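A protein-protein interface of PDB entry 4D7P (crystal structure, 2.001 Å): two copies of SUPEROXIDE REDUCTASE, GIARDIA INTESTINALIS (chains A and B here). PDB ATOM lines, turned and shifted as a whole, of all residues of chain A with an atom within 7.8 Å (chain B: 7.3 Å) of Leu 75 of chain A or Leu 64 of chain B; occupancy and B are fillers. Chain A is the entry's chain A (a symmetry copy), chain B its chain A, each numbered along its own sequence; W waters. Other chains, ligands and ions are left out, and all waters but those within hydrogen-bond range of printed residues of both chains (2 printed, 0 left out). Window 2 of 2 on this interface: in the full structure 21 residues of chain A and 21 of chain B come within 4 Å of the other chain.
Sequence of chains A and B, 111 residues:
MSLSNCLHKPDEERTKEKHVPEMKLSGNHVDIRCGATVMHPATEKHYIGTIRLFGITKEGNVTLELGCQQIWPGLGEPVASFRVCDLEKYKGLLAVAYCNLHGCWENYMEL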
ATOM      1  N   ALA A  42      -4.034  15.626  30.061  1.00  0.00           N
ATOM      2  CA  ALA A  42      -3.158  16.600  29.436  1.00  0.00           C
ATOM      3  C   ALA A  42      -1.777  15.981  29.290  1.00  0.00           C
ATOM      4  O   ALA A  42      -0.913  16.109  30.170  1.00  0.00           O
ATOM      5  CB  ALA A  42      -3.100  17.877  30.260  1.00  0.00           C
ATOM      6  N   THR A  43      -1.588  15.266  28.184  1.00  0.00           N
ATOM      7  CA  THR A  43      -0.322  14.607  27.892  1.00  0.00           C
ATOM      8  C   THR A  43       0.063  14.858  26.447  1.00  0.00           C
ATOM      9  O   THR A  43      -0.753  15.357  25.662  1.00  0.00           O
ATOM     10  CB  THR A  43      -0.393  13.076  28.124  1.00  0.00           C
ATOM     11  OG1 THR A  43      -1.216  12.486  27.112  1.00  0.00           O
ATOM     12  CG2 THR A  43      -0.979  12.755  29.500  1.00  0.00           C
ATOM     13  N   GLU A  44       1.293  14.489  26.090  1.00  0.00           N
ATOM     14  CA  GLU A  44       1.788  14.689  24.736  1.00  0.00           C
ATOM     15  C   GLU A  44       1.052  13.830  23.724  1.00  0.00           C
ATOM     16  O   GLU A  44       1.003  14.167  22.537  1.00  0.00           O
ATOM     17  CB  GLU A  44       3.283  14.407  24.672  1.00  0.00           C
ATOM     18  CG  GLU A  44       4.076  15.346  25.541  1.00  0.00           C
ATOM     19  CD  GLU A  44       5.567  15.172  25.387  1.00  0.00           C
ATOM     20  OE1 GLU A  44       6.007  14.053  25.033  1.00  0.00           O
ATOM     21  OE2 GLU A  44       6.300  16.161  25.619  1.00  0.00           O
ATOM     22  N   TYR A  47      -4.638  14.869  24.559  1.00  0.00           N
ATOM     23  CA  TYR A  47      -4.798  16.257  24.962  1.00  0.00           C
ATOM     24  C   TYR A  47      -6.034  16.901  24.351  1.00  0.00           C
ATOM     25  O   TYR A  47      -6.491  16.496  23.284  1.00  0.00           O
ATOM     26  CB  TYR A  47      -3.554  17.054  24.567  1.00  0.00           C
ATOM     27  CG  TYR A  47      -3.178  16.950  23.084  1.00  0.00           C
ATOM     28  CD1 TYR A  47      -3.688  17.851  22.164  1.00  0.00           C
ATOM     29  CD2 TYR A  47      -2.307  15.967  22.622  1.00  0.00           C
ATOM     30  CE1 TYR A  47      -3.352  17.781  20.826  1.00  0.00           C
ATOM     31  CE2 TYR A  47      -1.956  15.886  21.255  1.00  0.00           C
ATOM     32  CZ  TYR A  47      -2.493  16.811  20.371  1.00  0.00           C
ATOM     33  OH  TYR A  47      -2.181  16.784  19.022  1.00  0.00           O
ATOM     34  N   ILE A  71      -3.618  25.084  23.396  1.00  0.00           N
ATOM     35  CA  ILE A  71      -2.818  24.576  24.508  1.00  0.00           C
ATOM     36  C   ILE A  71      -1.840  23.523  24.010  1.00  0.00           C
ATOM     37  O   ILE A  71      -2.226  22.579  23.339  1.00  0.00           O
ATOM     38  CB  ILE A  71      -3.704  23.957  25.599  1.00  0.00           C
ATOM     39  CG1 ILE A  71      -4.791  24.952  26.015  1.00  0.00           C
ATOM     40  CG2 ILE A  71      -2.864  23.518  26.800  1.00  0.00           C
ATOM     41  CD1 ILE A  71      -5.938  24.315  26.765  1.00  0.00           C
ATOM     42  N   TRP A  72      -0.569  23.685  24.332  1.00  0.00           N
ATOM     43  CA  TRP A  72       0.412  22.711  23.880  1.00  0.00           C
ATOM     44  C   TRP A  72       0.262  21.420  24.672  1.00  0.00           C
ATOM     45  O   TRP A  72       0.122  21.445  25.893  1.00  0.00           O
ATOM     46  CB  TRP A  72       1.826  23.289  23.983  1.00  0.00           C
ATOM     47  CG  TRP A  72       2.027  24.387  22.963  1.00  0.00           C
ATOM     48  CD1 TRP A  72       2.137  25.721  23.204  1.00  0.00           C
ATOM     49  CD2 TRP A  72       2.087  24.227  21.533  1.00  0.00           C
ATOM     50  NE1 TRP A  72       2.279  26.410  22.012  1.00  0.00           N
ATOM     51  CE2 TRP A  72       2.245  25.515  20.977  1.00  0.00           C
ATOM     52  CE3 TRP A  72       2.027  23.117  20.676  1.00  0.00           C
ATOM     53  CZ2 TRP A  72       2.337  25.721  19.590  1.00  0.00           C
ATOM     54  CZ3 TRP A  72       2.123  23.322  19.312  1.00  0.00           C
ATOM     55  CH2 TRP A  72       2.271  24.614  18.780  1.00  0.00           C
ATOM     56  N   PRO A  73       0.263  20.285  23.965  1.00  0.00           N
ATOM     57  CA  PRO A  73       0.022  18.977  24.591  1.00  0.00           C
ATOM     58  C   PRO A  73       0.859  18.748  25.854  1.00  0.00           C
ATOM     59  O   PRO A  73       2.085  18.847  25.828  1.00  0.00           O
ATOM     60  CB  PRO A  73       0.400  17.993  23.484  1.00  0.00           C
ATOM     61  CG  PRO A  73       0.097  18.746  22.218  1.00  0.00           C
ATOM     62  CD  PRO A  73       0.482  20.171  22.510  1.00  0.00           C
ATOM     63  N   GLY A  74       0.174  18.478  26.961  1.00  0.00           N
ATOM     64  CA  GLY A  74       0.819  18.139  28.212  1.00  0.00           C
ATOM     65  C   GLY A  74       1.485  19.301  28.928  1.00  0.00           C
ATOM     66  O   GLY A  74       2.128  19.101  29.955  1.00  0.00           O
ATOM     67  N   LEU A  75       1.338  20.512  28.402  1.00  0.00           N
ATOM     68  CA  LEU A  75       1.937  21.681  29.045  1.00  0.00           C
ATOM     69  C   LEU A  75       0.910  22.491  29.830  1.00  0.00           C
ATOM     70  O   LEU A  75       1.260  23.264  30.733  1.00  0.00           O
ATOM     71  CB  LEU A  75       2.620  22.564  28.013  1.00  0.00           C
ATOM     72  CG  LEU A  75       3.763  21.852  27.292  1.00  0.00           C
ATOM     73  CD1 LEU A  75       4.563  22.813  26.426  1.00  0.00           C
ATOM     74  CD2 LEU A  75       4.657  21.143  28.310  1.00  0.00           C
ATOM     75  N   GLY A  76      -0.357  22.319  29.473  1.00  0.00           N
ATOM     76  CA  GLY A  76      -1.435  22.989  30.167  1.00  0.00           C
ATOM     77  C   GLY A  76      -2.664  22.110  30.176  1.00  0.00           C
ATOM     78  O   GLY A  76      -2.864  21.278  29.282  1.00  0.00           O
ATOM     79  N   GLU A  77      -3.496  22.301  31.191  1.00  0.00           N
ATOM     80  CA  GLU A  77      -4.770  21.594  31.296  1.00  0.00           C
ATOM     81  C   GLU A  77      -5.835  22.349  30.523  1.00  0.00           C
ATOM     82  O   GLU A  77      -5.666  23.538  30.287  1.00  0.00           O
ATOM     83  CB  GLU A  77      -5.160  21.453  32.763  1.00  0.00           C
ATOM     84  CG  GLU A  77      -4.070  20.781  33.570  1.00  0.00           C
ATOM     85  CD  GLU A  77      -4.549  20.380  34.936  1.00  0.00           C
ATOM     86  OE1 GLU A  77      -5.209  19.330  35.037  1.00  0.00           O
ATOM     87  OE2 GLU A  77      -4.269  21.111  35.903  1.00  0.00           O
ATOM     88  N   LEU B  53       1.235  32.437  27.257  1.00  0.00           N
ATOM     89  CA  LEU B  53       1.865  32.144  28.534  1.00  0.00           C
ATOM     90  C   LEU B  53       3.041  31.199  28.327  1.00  0.00           C
ATOM     91  O   LEU B  53       2.903  30.147  27.703  1.00  0.00           O
ATOM     92  CB  LEU B  53       0.863  31.530  29.529  1.00  0.00           C
ATOM     93  CG  LEU B  53       1.416  31.325  30.947  1.00  0.00           C
ATOM     94  CD1 LEU B  53       1.801  32.669  31.558  1.00  0.00           C
ATOM     95  CD2 LEU B  53       0.429  30.585  31.864  1.00  0.00           C
ATOM     96  N   PHE B  54       4.196  31.598  28.844  1.00  0.00           N
ATOM     97  CA  PHE B  54       5.408  30.791  28.783  1.00  0.00           C
ATOM     98  C   PHE B  54       5.821  30.348  30.178  1.00  0.00           C
ATOM     99  O   PHE B  54       5.704  31.116  31.135  1.00  0.00           O
ATOM    100  CB  PHE B  54       6.570  31.572  28.154  1.00  0.00           C
ATOM    101  CG  PHE B  54       6.334  31.999  26.738  1.00  0.00           C
ATOM    102  CD1 PHE B  54       5.685  33.194  26.458  1.00  0.00           C
ATOM    103  CD2 PHE B  54       6.790  31.227  25.687  1.00  0.00           C
ATOM    104  CE1 PHE B  54       5.468  33.588  25.155  1.00  0.00           C
ATOM    105  CE2 PHE B  54       6.576  31.622  24.372  1.00  0.00           C
ATOM    106  CZ  PHE B  54       5.913  32.797  24.110  1.00  0.00           C
ATOM    107  N   GLY B  55       6.307  29.114  30.292  1.00  0.00           N
ATOM    108  CA  GLY B  55       7.046  28.703  31.480  1.00  0.00           C
ATOM    109  C   GLY B  55       8.553  28.640  31.251  1.00  0.00           C
ATOM    110  O   GLY B  55       9.014  28.058  30.271  1.00  0.00           O
ATOM    111  N   ILE B  56       9.331  29.232  32.152  1.00  0.00           N
ATOM    112  CA  ILE B  56      10.785  29.105  32.090  1.00  0.00           C
ATOM    113  C   ILE B  56      11.218  27.887  32.905  1.00  0.00           C
ATOM    114  O   ILE B  56      11.016  27.840  34.125  1.00  0.00           O
ATOM    115  CB  ILE B  56      11.499  30.339  32.621  1.00  0.00           C
ATOM    116  CG1 ILE B  56      10.831  31.605  32.091  1.00  0.00           C
ATOM    117  CG2 ILE B  56      12.960  30.305  32.229  1.00  0.00           C
ATOM    118  CD1 ILE B  56      10.760  31.674  30.612  1.00  0.00           C
ATOM    119  N   THR B  57      11.809  26.905  32.231  1.00  0.00           N
ATOM    120  CA  THR B  57      12.124  25.630  32.865  1.00  0.00           C
ATOM    121  C   THR B  57      13.339  25.716  33.782  1.00  0.00           C
ATOM    122  O   THR B  57      14.303  26.427  33.490  1.00  0.00           O
ATOM    123  CB  THR B  57      12.385  24.537  31.818  1.00  0.00           C
ATOM    124  OG1 THR B  57      13.627  24.802  31.152  1.00  0.00           O
ATOM    125  CG2 THR B  57      11.257  24.501  30.796  1.00  0.00           C
ATOM    126  N   ASN B  61      16.708  25.972  31.470  1.00  0.00           N
ATOM    127  CA  ASN B  61      16.457  27.394  31.223  1.00  0.00           C
ATOM    128  C   ASN B  61      15.736  27.663  29.901  1.00  0.00           C
ATOM    129  O   ASN B  61      16.022  28.640  29.200  1.00  0.00           O
ATOM    130  CB  ASN B  61      17.761  28.181  31.248  1.00  0.00           C
ATOM    131  CG  ASN B  61      17.527  29.666  31.334  1.00  0.00           C
ATOM    132  OD1 ASN B  61      16.723  30.128  32.143  1.00  0.00           O
ATOM    133  ND2 ASN B  61      18.188  30.424  30.468  1.00  0.00           N
ATOM    134  N   VAL B  62      14.797  26.795  29.556  1.00  0.00           N
ATOM    135  CA  VAL B  62      14.058  26.949  28.306  1.00  0.00           C
ATOM    136  C   VAL B  62      12.857  27.856  28.515  1.00  0.00           C
ATOM    137  O   VAL B  62      12.233  27.819  29.562  1.00  0.00           O
ATOM    138  CB  VAL B  62      13.611  25.574  27.765  1.00  0.00           C
ATOM    139  CG1 VAL B  62      12.792  25.709  26.475  1.00  0.00           C
ATOM    140  CG2 VAL B  62      14.839  24.674  27.550  1.00  0.00           C
ATOM    141  N   THR B  63      12.553  28.688  27.526  1.00  0.00           N
ATOM    142  CA  THR B  63      11.335  29.492  27.553  1.00  0.00           C
ATOM    143  C   THR B  63      10.237  28.767  26.771  1.00  0.00           C
ATOM    144  O   THR B  63      10.121  28.901  25.552  1.00  0.00           O
ATOM    145  CB  THR B  63      11.578  30.894  26.975  1.00  0.00           C
ATOM    146  OG1 THR B  63      12.571  31.561  27.764  1.00  0.00           O
ATOM    147  CG2 THR B  63      10.304  31.713  27.000  1.00  0.00           C
ATOM    148  N   LEU B  64       9.456  27.965  27.484  1.00  0.00           N
ATOM    149  CA  LEU B  64       8.540  27.019  26.860  1.00  0.00           C
ATOM    150  C   LEU B  64       7.108  27.574  26.758  1.00  0.00           C
ATOM    151  O   LEU B  64       6.496  27.894  27.774  1.00  0.00           O
ATOM    152  CB  LEU B  64       8.548  25.723  27.669  1.00  0.00           C
ATOM    153  CG  LEU B  64       7.740  24.517  27.208  1.00  0.00           C
ATOM    154  CD1 LEU B  64       8.284  23.967  25.885  1.00  0.00           C
ATOM    155  CD2 LEU B  64       7.761  23.445  28.291  1.00  0.00           C
ATOM    156  N   GLU B  65       6.575  27.697  25.546  1.00  0.00           N
ATOM    157  CA  GLU B  65       5.221  28.215  25.396  1.00  0.00           C
ATOM    158  C   GLU B  65       4.227  27.170  25.847  1.00  0.00           C
ATOM    159  O   GLU B  65       4.210  26.049  25.343  1.00  0.00           O
ATOM    160  CB  GLU B  65       4.918  28.634  23.957  1.00  0.00           C
ATOM    161  CG  GLU B  65       3.589  29.387  23.863  1.00  0.00           C
ATOM    162  CD  GLU B  65       3.223  29.787  22.450  1.00  0.00           C
ATOM    163  OE1 GLU B  65       3.782  30.772  21.935  1.00  0.00           O
ATOM    164  OE2 GLU B  65       2.370  29.115  21.849  1.00  0.00           O
ATOM    165  N   LEU B  66       3.409  27.536  26.819  1.00  0.00           N
ATOM    166  CA  LEU B  66       2.427  26.613  27.354  1.00  0.00           C
ATOM    167  C   LEU B  66       1.164  26.649  26.531  1.00  0.00           C
ATOM    168  O   LEU B  66       0.500  25.619  26.362  1.00  0.00           O
ATOM    169  CB  LEU B  66       2.120  26.944  28.817  1.00  0.00           C
ATOM    170  CG  LEU B  66       3.377  27.126  29.678  1.00  0.00           C
ATOM    171  CD1 LEU B  66       2.974  27.515  31.078  1.00  0.00           C
ATOM    172  CD2 LEU B  66       4.214  25.849  29.685  1.00  0.00           C
ATOM    173  N   GLY B  67       0.826  27.832  26.020  1.00  0.00           N
ATOM    174  CA  GLY B  67      -0.352  27.970  25.177  1.00  0.00           C
ATOM    175  C   GLY B  67      -0.574  29.404  24.728  1.00  0.00           C
ATOM    176  O   GLY B  67       0.195  30.294  25.084  1.00  0.00           O
ATOM    177  N   PHE B  82      -4.949  29.905  32.023  1.00  0.00           N
ATOM    178  CA  PHE B  82      -4.198  28.693  31.775  1.00  0.00           C
ATOM    179  C   PHE B  82      -4.177  27.881  33.035  1.00  0.00           C
ATOM    180  O   PHE B  82      -4.467  28.386  34.120  1.00  0.00           O
ATOM    181  CB  PHE B  82      -2.778  29.012  31.350  1.00  0.00           C
ATOM    182  CG  PHE B  82      -2.698  29.834  30.106  1.00  0.00           C
ATOM    183  CD1 PHE B  82      -2.936  31.195  30.141  1.00  0.00           C
ATOM    184  CD2 PHE B  82      -2.388  29.243  28.889  1.00  0.00           C
ATOM    185  CE1 PHE B  82      -2.859  31.959  28.991  1.00  0.00           C
ATOM    186  CE2 PHE B  82      -2.306  30.000  27.744  1.00  0.00           C
ATOM    187  CZ  PHE B  82      -2.548  31.364  27.795  1.00  0.00           C
ATOM    188  N   ARG B  83      -3.829  26.615  32.905  1.00  0.00           N
ATOM    189  CA  ARG B  83      -3.602  25.823  34.092  1.00  0.00           C
ATOM    190  C   ARG B  83      -2.339  25.035  33.836  1.00  0.00           C
ATOM    191  O   ARG B  83      -2.315  24.134  33.008  1.00  0.00           O
ATOM    192  CB  ARG B  83      -4.793  24.927  34.391  1.00  0.00           C
ATOM    193  CG  ARG B  83      -4.758  24.315  35.775  1.00  0.00           C
ATOM    194  CD  ARG B  83      -6.114  23.781  36.169  1.00  0.00           C
ATOM    195  NE  ARG B  83      -6.589  24.416  37.387  1.00  0.00           N
ATOM    196  CZ  ARG B  83      -7.764  25.016  37.517  1.00  0.00           C
ATOM    197  NH1 ARG B  83      -8.607  25.064  36.501  1.00  0.00           N
ATOM    198  NH2 ARG B  83      -8.095  25.569  38.676  1.00  0.00           N
ATOM    199  N   VAL B  84      -1.281  25.405  34.536  1.00  0.00           N
ATOM    200  CA  VAL B  84       0.036  24.911  34.206  1.00  0.00           C
ATOM    201  C   VAL B  84       0.278  23.494  34.700  1.00  0.00           C
ATOM    202  O   VAL B  84       0.236  23.220  35.892  1.00  0.00           O
ATOM    203  CB  VAL B  84       1.122  25.838  34.774  1.00  0.00           C
ATOM    204  CG1 VAL B  84       2.505  25.280  34.463  1.00  0.00           C
ATOM    205  CG2 VAL B  84       0.962  27.234  34.195  1.00  0.00           C
ATOM    206  N   CYS B  85       0.543  22.589  33.768  1.00  0.00           N
ATOM    207  CA  CYS B  85       0.930  21.230  34.132  1.00  0.00           C
ATOM    208  C   CYS B  85       2.255  21.224  34.855  1.00  0.00           C
ATOM    209  O   CYS B  85       3.169  21.938  34.452  1.00  0.00           O
ATOM    210  CB  CYS B  85       1.034  20.349  32.892  1.00  0.00           C
ATOM    211  SG  CYS B  85      -0.525  20.055  32.087  1.00  0.00           S
ATOM    212  N   ASP B  86       2.362  20.423  35.914  1.00  0.00           N
ATOM    213  CA  ASP B  86       3.643  20.239  36.584  1.00  0.00           C
ATOM    214  C   ASP B  86       4.327  21.582  36.877  1.00  0.00           C
ATOM    215  O   ASP B  86       5.445  21.811  36.411  1.00  0.00           O
ATOM    216  CB  ASP B  86       4.564  19.373  35.719  1.00  0.00           C
ATOM    217  CG  ASP B  86       3.954  18.023  35.372  1.00  0.00           C
ATOM    218  OD1 ASP B  86       3.350  17.389  36.264  1.00  0.00           O
ATOM    219  OD2 ASP B  86       4.077  17.593  34.205  1.00  0.00           O
ATOM    220  N   TYR B  90       8.916  24.656  36.711  1.00  0.00           N
ATOM    221  CA  TYR B  90       9.317  25.967  36.207  1.00  0.00           C
ATOM    222  C   TYR B  90       9.794  26.889  37.314  1.00  0.00           C
ATOM    223  O   TYR B  90       9.381  26.753  38.465  1.00  0.00           O
ATOM    224  CB  TYR B  90       8.154  26.638  35.452  1.00  0.00           C
ATOM    225  CG  TYR B  90       7.561  25.772  34.366  1.00  0.00           C
ATOM    226  CD1 TYR B  90       8.095  25.765  33.080  1.00  0.00           C
ATOM    227  CD2 TYR B  90       6.473  24.944  34.630  1.00  0.00           C
ATOM    228  CE1 TYR B  90       7.559  24.965  32.086  1.00  0.00           C
ATOM    229  CE2 TYR B  90       5.926  24.145  33.643  1.00  0.00           C
ATOM    230  CZ  TYR B  90       6.472  24.160  32.372  1.00  0.00           C
ATOM    231  OH  TYR B  90       5.919  23.363  31.394  1.00  0.00           O
ATOM    232  N   LEU B  94       6.023  33.684  32.150  1.00  0.00           N
ATOM    233  CA  LEU B  94       6.132  34.876  31.321  1.00  0.00           C
ATOM    234  C   LEU B  94       4.876  35.014  30.481  1.00  0.00           C
ATOM    235  O   LEU B  94       4.596  34.156  29.645  1.00  0.00           O
ATOM    236  CB  LEU B  94       7.372  34.804  30.413  1.00  0.00           C
ATOM    237  CG  LEU B  94       7.509  35.919  29.372  1.00  0.00           C
ATOM    238  CD1 LEU B  94       7.803  37.261  30.044  1.00  0.00           C
ATOM    239  CD2 LEU B  94       8.556  35.579  28.316  1.00  0.00           C
HETATM  240  O   HOH W   1      -3.965  25.679  30.164  1.00  0.00           O
HETATM  241  O   HOH W   2       3.588  22.456  31.897  1.00  0.00           O
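N of Leu 53 of chain B is in hydrogen-bond range of O of Gly 67 of chain B (3.2 Å). The backbone carbonyl oxygen (O) of Leu 53 of chain B is in hydrogen-bond range of the backbone NH (N) of Leu 66 of chain B (2.8 Å). N of Gly 55 of chain B lies within hydrogen-bond range of O of Leu 64 of chain B, 2.8 Å away.
Leu 64 of chain B touches just one residue of chain A: Leu 75 (3.7 Å). Gly 74 of chain A touches just one residue of chain B: Cys 85 (3.4 Å). Printed residues of chain A within 4 Å of Cys 85 of chain B: Ala 42 (3.8 Å), Gly 74 (3.4 Å), Leu 75 (3.2 Å), Gly 76 (3.5 Å) and Glu 77 (3.8 Å). Of the printed residues of chain A, Gly 67 of chain B touches Trp 72 (3.8 Å). Of the printed residues of chain B, Trp 72 of chain A touches Glu 65, Leu 66 and Gly 67. The nearest residue of chain A that does not touch Leu 64 of chain B is Trp 72 of chain A (6.4 Å). The nearest printed residue of chain A that does not touch Gly 67 of chain B is Ile 71 of chain A (4.2 Å).
No position is printed for both chains. Of the 13 pairs that touch across the chains among the printed residues, none has its exchanged pair printed and touching as well.
The side-chain sulfur (SG) of Cys 85 of chain B is in hydrogen-bond range of the backbone NH (N) of Gly 76 of chain A (3.5 Å). The side-chain carboxylate (OE2) of Glu 65 of chain B sits at hydrogen-bond distance from the indole nitrogen (NE1) of Trp 72 of chain A, 2.7 Å away. The backbone NH of Cys 85 of chain B is in hydrogen-bond range of the backbone carbonyl oxygen of Leu 75 of chain A (3.2 Å). N of Trp 72 of chain A is in hydrogen-bond range of O of Leu 66 of chain B (3.0 Å). O of Gly 74 of chain A lies close to SG of Cys 85 of chain B (3.5 Å). The backbone NH of Glu 77 of chain A is in hydrogen-bond range of the backbone carbonyl oxygen of Arg 83 of chain B, 2.8 Å away.
Water W2 lies within hydrogen-bond range of OH of Tyr 90 of chain B (2.6 Å), O of Cys 85 of chain B (2.6 Å) and O of Leu 75 of chain A (2.7 Å). Water W1 lies within hydrogen-bond range of O of Glu 77 of chain A (2.7 Å) and N of Arg 83 of chain B (2.9 Å).
Of the 11 printed residues of chain A, 7 touch a printed residue of chain B. Printed residues of chain A that touch a printed residue of chain B: Ala 42, Ile 71, Trp 72, Gly 74, Leu 75, Gly 76 and Glu 77. Along chain A the printed residues that touch a printed residue of chain B span positions 42 to 77. Printed residues of chain B that touch a printed residue of chain A: Leu 64, Glu 65, Leu 66, Gly 67, Arg 83 and Cys 85. Hydrophobic or aromatic side chains of chain B within 4 Å of the printed part of chain A: Leu 64. Among the printed residues, 13 pairs touch across the chains.
Ala 42 of chain A touches Cys 85 of chain B. Ile 71 of chain A touches Leu 66 of chain B (C to O, 3.9 Å). Trp 72 of chain A touches Gly 67 of chain B (CD1 to N, 3.8 Å). Leu 64 of chain B touches Leu 75 of chain A. Glu 65 of chain B touches Leu 75 of chain A (O to CD1, 3.4 Å). Arg 83 of chain B touches Gly 76 of chain A. Glu 77 of chain A touches Cys 85 of chain B (N to SG, 3.8 Å).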
